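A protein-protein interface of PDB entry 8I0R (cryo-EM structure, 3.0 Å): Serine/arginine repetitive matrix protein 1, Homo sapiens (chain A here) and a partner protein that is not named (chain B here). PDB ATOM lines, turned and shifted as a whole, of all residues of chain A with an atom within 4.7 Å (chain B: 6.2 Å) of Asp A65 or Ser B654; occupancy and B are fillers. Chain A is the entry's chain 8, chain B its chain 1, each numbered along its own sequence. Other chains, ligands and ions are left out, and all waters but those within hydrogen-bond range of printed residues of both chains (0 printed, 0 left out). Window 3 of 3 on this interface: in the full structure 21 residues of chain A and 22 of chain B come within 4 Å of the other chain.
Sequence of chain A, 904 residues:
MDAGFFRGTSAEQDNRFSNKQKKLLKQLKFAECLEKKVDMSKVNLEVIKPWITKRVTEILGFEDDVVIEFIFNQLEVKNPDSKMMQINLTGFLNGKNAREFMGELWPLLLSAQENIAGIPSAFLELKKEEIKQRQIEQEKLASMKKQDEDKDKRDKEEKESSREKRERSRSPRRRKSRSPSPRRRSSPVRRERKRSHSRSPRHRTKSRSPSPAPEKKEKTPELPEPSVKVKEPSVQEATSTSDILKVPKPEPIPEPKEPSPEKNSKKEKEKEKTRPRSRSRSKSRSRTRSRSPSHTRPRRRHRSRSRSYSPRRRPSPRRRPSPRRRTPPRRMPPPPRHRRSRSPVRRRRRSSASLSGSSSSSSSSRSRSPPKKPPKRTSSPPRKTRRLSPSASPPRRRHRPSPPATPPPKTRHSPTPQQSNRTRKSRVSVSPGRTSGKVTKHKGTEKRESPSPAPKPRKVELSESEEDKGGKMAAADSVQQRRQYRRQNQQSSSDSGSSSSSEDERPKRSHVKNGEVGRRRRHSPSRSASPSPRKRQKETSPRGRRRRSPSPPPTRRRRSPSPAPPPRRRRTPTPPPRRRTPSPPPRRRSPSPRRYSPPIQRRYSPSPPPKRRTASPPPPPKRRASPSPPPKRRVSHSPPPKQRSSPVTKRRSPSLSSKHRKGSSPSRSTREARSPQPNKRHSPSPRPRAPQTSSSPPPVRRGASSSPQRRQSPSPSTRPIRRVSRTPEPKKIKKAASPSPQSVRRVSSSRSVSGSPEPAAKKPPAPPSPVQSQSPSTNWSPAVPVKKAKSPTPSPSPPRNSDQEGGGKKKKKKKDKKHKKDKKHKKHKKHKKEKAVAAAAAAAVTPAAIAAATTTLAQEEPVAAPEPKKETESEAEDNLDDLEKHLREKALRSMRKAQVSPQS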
ATOM      1  N   GLU A  63      10.456   9.024   7.441  1.00  0.00           N
ATOM      2  CA  GLU A  63      11.818   9.417   7.767  1.00  0.00           C
ATOM      3  C   GLU A  63      12.300   8.603   8.956  1.00  0.00           C
ATOM      4  O   GLU A  63      11.583   8.469   9.952  1.00  0.00           O
ATOM      5  CB  GLU A  63      11.896  10.909   8.087  1.00  0.00           C
ATOM      6  CG  GLU A  63      10.822  11.414   9.037  1.00  0.00           C
ATOM      7  CD  GLU A  63       9.454  11.528   8.394  1.00  0.00           C
ATOM      8  OE1 GLU A  63       9.361  11.359   7.162  1.00  0.00           O
ATOM      9  OE2 GLU A  63       8.470  11.779   9.120  1.00  0.00           O
ATOM     10  N   ASP A  64      13.511   8.053   8.850  1.00  0.00           N
ATOM     11  CA  ASP A  64      14.100   7.291   9.950  1.00  0.00           C
ATOM     12  C   ASP A  64      15.500   7.844  10.200  1.00  0.00           C
ATOM     13  O   ASP A  64      16.497   7.339   9.670  1.00  0.00           O
ATOM     14  CB  ASP A  64      14.116   5.804   9.659  1.00  0.00           C
ATOM     15  CG  ASP A  64      14.042   4.975  10.920  1.00  0.00           C
ATOM     16  OD1 ASP A  64      13.629   3.802  10.844  1.00  0.00           O
ATOM     17  OD2 ASP A  64      14.382   5.506  11.994  1.00  0.00           O
ATOM     18  N   ASP A  65      15.538   8.887  11.032  1.00  0.00           N
ATOM     19  CA  ASP A  65      16.782   9.485  11.499  1.00  0.00           C
ATOM     20  C   ASP A  65      17.848   8.447  11.791  1.00  0.00           C
ATOM     21  O   ASP A  65      19.015   8.640  11.447  1.00  0.00           O
ATOM     22  CB  ASP A  65      16.497  10.310  12.744  1.00  0.00           C
ATOM     23  CG  ASP A  65      15.636   9.568  13.718  1.00  0.00           C
ATOM     24  OD1 ASP A  65      14.484   9.260  13.357  1.00  0.00           O
ATOM     25  OD2 ASP A  65      16.110   9.265  14.829  1.00  0.00           O
ATOM     26  N   VAL A  66      17.486   7.372  12.488  1.00  0.00           N
ATOM     27  CA  VAL A  66      18.494   6.415  12.918  1.00  0.00           C
ATOM     28  C   VAL A  66      19.113   5.707  11.725  1.00  0.00           C
ATOM     29  O   VAL A  66      20.321   5.470  11.698  1.00  0.00           O
ATOM     30  CB  VAL A  66      17.887   5.420  13.911  1.00  0.00           C
ATOM     31  CG1 VAL A  66      18.946   4.453  14.385  1.00  0.00           C
ATOM     32  CG2 VAL A  66      17.278   6.169  15.071  1.00  0.00           C
ATOM     33  N   VAL A  67      18.319   5.374  10.712  1.00  0.00           N
ATOM     34  CA  VAL A  67      18.910   4.785   9.515  1.00  0.00           C
ATOM     35  C   VAL A  67      19.780   5.807   8.802  1.00  0.00           C
ATOM     36  O   VAL A  67      20.858   5.479   8.282  1.00  0.00           O
ATOM     37  CB  VAL A  67      17.821   4.225   8.589  1.00  0.00           C
ATOM     38  CG1 VAL A  67      18.437   3.255   7.613  1.00  0.00           C
ATOM     39  CG2 VAL A  67      16.761   3.540   9.400  1.00  0.00           C
ATOM     40  N   ILE A  68      19.337   7.067   8.783  1.00  0.00           N
ATOM     41  CA  ILE A  68      20.162   8.126   8.205  1.00  0.00           C
ATOM     42  C   ILE A  68      21.535   8.120   8.860  1.00  0.00           C
ATOM     43  O   ILE A  68      22.563   7.875   8.218  1.00  0.00           O
ATOM     44  CB  ILE A  68      19.494   9.497   8.392  1.00  0.00           C
ATOM     45  CG1 ILE A  68      17.991   9.433   8.185  1.00  0.00           C
ATOM     46  CG2 ILE A  68      20.038  10.472   7.411  1.00  0.00           C
ATOM     47  CD1 ILE A  68      17.591   9.064   6.837  1.00  0.00           C
ATOM     48  N   GLU A  69      21.550   8.359  10.168  1.00  0.00           N
ATOM     49  CA  GLU A  69      22.795   8.482  10.907  1.00  0.00           C
ATOM     50  C   GLU A  69      23.599   7.204  10.873  1.00  0.00           C
ATOM     51  O   GLU A  69      24.825   7.258  10.953  1.00  0.00           O
ATOM     52  CB  GLU A  69      22.517   8.882  12.347  1.00  0.00           C
ATOM     53  CG  GLU A  69      21.568  10.038  12.456  1.00  0.00           C
ATOM     54  CD  GLU A  69      22.238  11.350  12.150  1.00  0.00           C
ATOM     55  OE1 GLU A  69      23.437  11.485  12.468  1.00  0.00           O
ATOM     56  OE2 GLU A  69      21.572  12.241  11.583  1.00  0.00           O
ATOM     57  N   ARG B 614      15.662  -2.321  16.704  1.00  0.00           N
ATOM     58  CA  ARG B 614      15.637  -0.866  16.568  1.00  0.00           C
ATOM     59  C   ARG B 614      14.292  -0.260  16.936  1.00  0.00           C
ATOM     60  O   ARG B 614      14.262   0.701  17.722  1.00  0.00           O
ATOM     61  CB  ARG B 614      16.033  -0.438  15.161  1.00  0.00           C
ATOM     62  CG  ARG B 614      16.265   1.049  15.158  1.00  0.00           C
ATOM     63  CD  ARG B 614      15.101   1.807  14.578  1.00  0.00           C
ATOM     64  NE  ARG B 614      14.955   3.104  15.216  1.00  0.00           N
ATOM     65  CZ  ARG B 614      13.998   3.965  14.908  1.00  0.00           C
ATOM     66  NH1 ARG B 614      13.117   3.652  13.978  1.00  0.00           N
ATOM     67  NH2 ARG B 614      13.919   5.129  15.525  1.00  0.00           N
ATOM     68  N   ASP B 618      12.599   3.361  20.485  1.00  0.00           N
ATOM     69  CA  ASP B 618      11.643   4.450  20.448  1.00  0.00           C
ATOM     70  C   ASP B 618      10.290   4.072  21.015  1.00  0.00           C
ATOM     71  O   ASP B 618       9.334   4.832  20.842  1.00  0.00           O
ATOM     72  CB  ASP B 618      11.486   4.931  19.010  1.00  0.00           C
ATOM     73  CG  ASP B 618      12.819   5.280  18.368  1.00  0.00           C
ATOM     74  OD1 ASP B 618      13.870   4.868  18.906  1.00  0.00           O
ATOM     75  OD2 ASP B 618      12.815   5.956  17.319  1.00  0.00           O
ATOM     76  N   LYS B 649      26.175   5.532  18.333  1.00  0.00           N
ATOM     77  CA  LYS B 649      26.326   6.944  17.998  1.00  0.00           C
ATOM     78  C   LYS B 649      25.037   7.479  17.405  1.00  0.00           C
ATOM     79  O   LYS B 649      24.493   8.489  17.866  1.00  0.00           O
ATOM     80  CB  LYS B 649      27.469   7.163  17.009  1.00  0.00           C
ATOM     81  CG  LYS B 649      28.850   7.160  17.625  1.00  0.00           C
ATOM     82  CD  LYS B 649      29.768   8.131  16.913  1.00  0.00           C
ATOM     83  CE  LYS B 649      29.295   9.563  17.140  1.00  0.00           C
ATOM     84  NZ  LYS B 649      30.396  10.563  17.194  1.00  0.00           N
ATOM     85  N   ALA B 650      24.525   6.754  16.414  1.00  0.00           N
ATOM     86  CA  ALA B 650      23.266   7.124  15.787  1.00  0.00           C
ATOM     87  C   ALA B 650      22.176   7.363  16.821  1.00  0.00           C
ATOM     88  O   ALA B 650      21.692   8.488  16.976  1.00  0.00           O
ATOM     89  CB  ALA B 650      22.851   6.036  14.802  1.00  0.00           C
ATOM     90  N   VAL B 651      21.797   6.321  17.557  1.00  0.00           N
ATOM     91  CA  VAL B 651      20.603   6.415  18.396  1.00  0.00           C
ATOM     92  C   VAL B 651      20.780   7.485  19.467  1.00  0.00           C
ATOM     93  O   VAL B 651      19.874   8.282  19.729  1.00  0.00           O
ATOM     94  CB  VAL B 651      20.246   5.048  19.004  1.00  0.00           C
ATOM     95  CG1 VAL B 651      19.896   4.084  17.920  1.00  0.00           C
ATOM     96  CG2 VAL B 651      21.375   4.493  19.812  1.00  0.00           C
ATOM     97  N   CYS B 652      21.953   7.524  20.101  1.00  0.00           N
ATOM     98  CA  CYS B 652      22.148   8.439  21.218  1.00  0.00           C
ATOM     99  C   CYS B 652      22.324   9.877  20.742  1.00  0.00           C
ATOM    100  O   CYS B 652      22.285  10.810  21.550  1.00  0.00           O
ATOM    101  CB  CYS B 652      23.338   7.986  22.059  1.00  0.00           C
ATOM    102  SG  CYS B 652      24.617   9.205  22.364  1.00  0.00           S
ATOM    103  N   LYS B 653      22.519  10.083  19.437  1.00  0.00           N
ATOM    104  CA  LYS B 653      22.525  11.433  18.892  1.00  0.00           C
ATOM    105  C   LYS B 653      21.270  11.749  18.101  1.00  0.00           C
ATOM    106  O   LYS B 653      21.182  12.824  17.502  1.00  0.00           O
ATOM    107  CB  LYS B 653      23.758  11.662  18.021  1.00  0.00           C
ATOM    108  CG  LYS B 653      24.990  12.133  18.783  1.00  0.00           C
ATOM    109  CD  LYS B 653      25.604  13.348  18.109  1.00  0.00           C
ATOM    110  CE  LYS B 653      27.011  13.070  17.626  1.00  0.00           C
ATOM    111  NZ  LYS B 653      27.531  14.188  16.794  1.00  0.00           N
ATOM    112  N   SER B 654      20.306  10.834  18.067  1.00  0.00           N
ATOM    113  CA  SER B 654      19.009  11.157  17.492  1.00  0.00           C
ATOM    114  C   SER B 654      18.421  12.391  18.174  1.00  0.00           C
ATOM    115  O   SER B 654      18.419  12.520  19.398  1.00  0.00           O
ATOM    116  CB  SER B 654      18.053   9.975  17.635  1.00  0.00           C
ATOM    117  OG  SER B 654      16.717  10.400  17.827  1.00  0.00           O
ATOM    118  N   LYS B 655      17.896  13.300  17.358  1.00  0.00           N
ATOM    119  CA  LYS B 655      17.528  14.618  17.843  1.00  0.00           C
ATOM    120  C   LYS B 655      16.032  14.861  17.938  1.00  0.00           C
ATOM    121  O   LYS B 655      15.629  15.796  18.635  1.00  0.00           O
ATOM    122  CB  LYS B 655      18.142  15.705  16.948  1.00  0.00           C
ATOM    123  CG  LYS B 655      18.008  15.418  15.469  1.00  0.00           C
ATOM    124  CD  LYS B 655      17.690  16.671  14.681  1.00  0.00           C
ATOM    125  CE  LYS B 655      16.230  17.044  14.815  1.00  0.00           C
ATOM    126  NZ  LYS B 655      15.328  15.934  14.434  1.00  0.00           N
ATOM    127  N   LYS B 656      15.202  14.082  17.254  1.00  0.00           N
ATOM    128  CA  LYS B 656      13.764  14.222  17.433  1.00  0.00           C
ATOM    129  C   LYS B 656      13.354  13.844  18.852  1.00  0.00           C
ATOM    130  O   LYS B 656      12.758  14.645  19.579  1.00  0.00           O
ATOM    131  CB  LYS B 656      13.015  13.379  16.403  1.00  0.00           C
ATOM    132  CG  LYS B 656      11.502  13.541  16.484  1.00  0.00           C
ATOM    133  CD  LYS B 656      10.996  14.656  15.580  1.00  0.00           C
ATOM    134  CE  LYS B 656      10.582  14.126  14.215  1.00  0.00           C
ATOM    135  NZ  LYS B 656       9.185  13.602  14.199  1.00  0.00           N
ATOM    136  N   SER B 657      13.691  12.627  19.271  1.00  0.00           N
ATOM    137  CA  SER B 657      13.151  12.056  20.496  1.00  0.00           C
ATOM    138  C   SER B 657      14.232  11.962  21.559  1.00  0.00           C
ATOM    139  O   SER B 657      15.324  11.451  21.313  1.00  0.00           O
ATOM    140  CB  SER B 657      12.571  10.658  20.251  1.00  0.00           C
ATOM    141  OG  SER B 657      12.401   9.964  21.474  1.00  0.00           O
ATOM    142  N   TRP B 658      13.913  12.454  22.753  1.00  0.00           N
ATOM    143  CA  TRP B 658      14.846  12.285  23.853  1.00  0.00           C
ATOM    144  C   TRP B 658      14.747  10.907  24.472  1.00  0.00           C
ATOM    145  O   TRP B 658      15.659  10.510  25.195  1.00  0.00           O
ATOM    146  CB  TRP B 658      14.622  13.346  24.924  1.00  0.00           C
ATOM    147  CG  TRP B 658      13.396  13.156  25.719  1.00  0.00           C
ATOM    148  CD1 TRP B 658      12.196  13.755  25.529  1.00  0.00           C
ATOM    149  CD2 TRP B 658      13.246  12.300  26.845  1.00  0.00           C
ATOM    150  NE1 TRP B 658      11.300  13.324  26.471  1.00  0.00           N
ATOM    151  CE2 TRP B 658      11.926  12.427  27.292  1.00  0.00           C
ATOM    152  CE3 TRP B 658      14.106  11.436  27.524  1.00  0.00           C
ATOM    153  CZ2 TRP B 658      11.450  11.733  28.388  1.00  0.00           C
ATOM    154  CZ3 TRP B 658      13.629  10.738  28.593  1.00  0.00           C
ATOM    155  CH2 TRP B 658      12.314  10.886  29.019  1.00  0.00           C
ATOM    156  N   ALA B 660      14.980   8.161  22.792  1.00  0.00           N
ATOM    157  CA  ALA B 660      16.062   7.433  22.148  1.00  0.00           C
ATOM    158  C   ALA B 660      17.408   7.849  22.716  1.00  0.00           C
ATOM    159  O   ALA B 660      18.305   7.021  22.884  1.00  0.00           O
ATOM    160  CB  ALA B 660      16.012   7.650  20.640  1.00  0.00           C
ATOM    161  N   ARG B 661      17.567   9.130  23.031  1.00  0.00           N
ATOM    162  CA  ARG B 661      18.818   9.560  23.634  1.00  0.00           C
ATOM    163  C   ARG B 661      19.007   8.912  24.994  1.00  0.00           C
ATOM    164  O   ARG B 661      20.077   8.367  25.295  1.00  0.00           O
ATOM    165  CB  ARG B 661      18.849  11.081  23.739  1.00  0.00           C
ATOM    166  CG  ARG B 661      19.582  11.702  22.572  1.00  0.00           C
ATOM    167  CD  ARG B 661      19.613  13.202  22.607  1.00  0.00           C
ATOM    168  NE  ARG B 661      18.288  13.779  22.466  1.00  0.00           N
ATOM    169  CZ  ARG B 661      17.821  14.737  23.250  1.00  0.00           C
ATOM    170  NH1 ARG B 661      18.587  15.213  24.215  1.00  0.00           N
ATOM    171  NH2 ARG B 661      16.603  15.220  23.072  1.00  0.00           N
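Val A66 touches Arg B614.
Val A66 touches Val B651.
Ala B650 touches Glu A69.
NH1 of Arg B614 lies within salt-bridge range of OD2 of Asp A64, 3.0 Å away.
The side-chain hydroxyl of Ser B654 sits at hydrogen-bond distance from the side-chain carboxylate of Asp A65.
The side-chain carboxylate (OD1) of Asp B618 lies within salt-bridge range of the guanidinium group (NH2) of Arg B614, at 3.4 Å.
The backbone carbonyl oxygen (O) of Ser B654 is in hydrogen-bond range of the guanidinium group (NE) of Arg B661 (3.3 Å).
Of the 7 printed residues of chain A, 4 touch a printed residue of chain B.
Hydrophobic or aromatic side chains of chain B within 4 Å of the printed part of chain A: Ala B650 and Val B651.
Ser B654 touches one residue of chain A.
Of the printed residues of chain B, Glu A69 touches Ala B650 (3.8 Å).
Of the printed residues of chain B, Val A66 touches Arg B614 and Val B651.
Printed residues of chain A within 4 Å of Ala B650: Glu A69.
Printed residues of chain A within 4 Å of Val B651: Val A66.
Printed residues of chain B within 4 Å of Asp A64: Arg B614.
The nearest printed residue of chain A that does not touch Val B651 is Glu A69 (5.8 Å).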
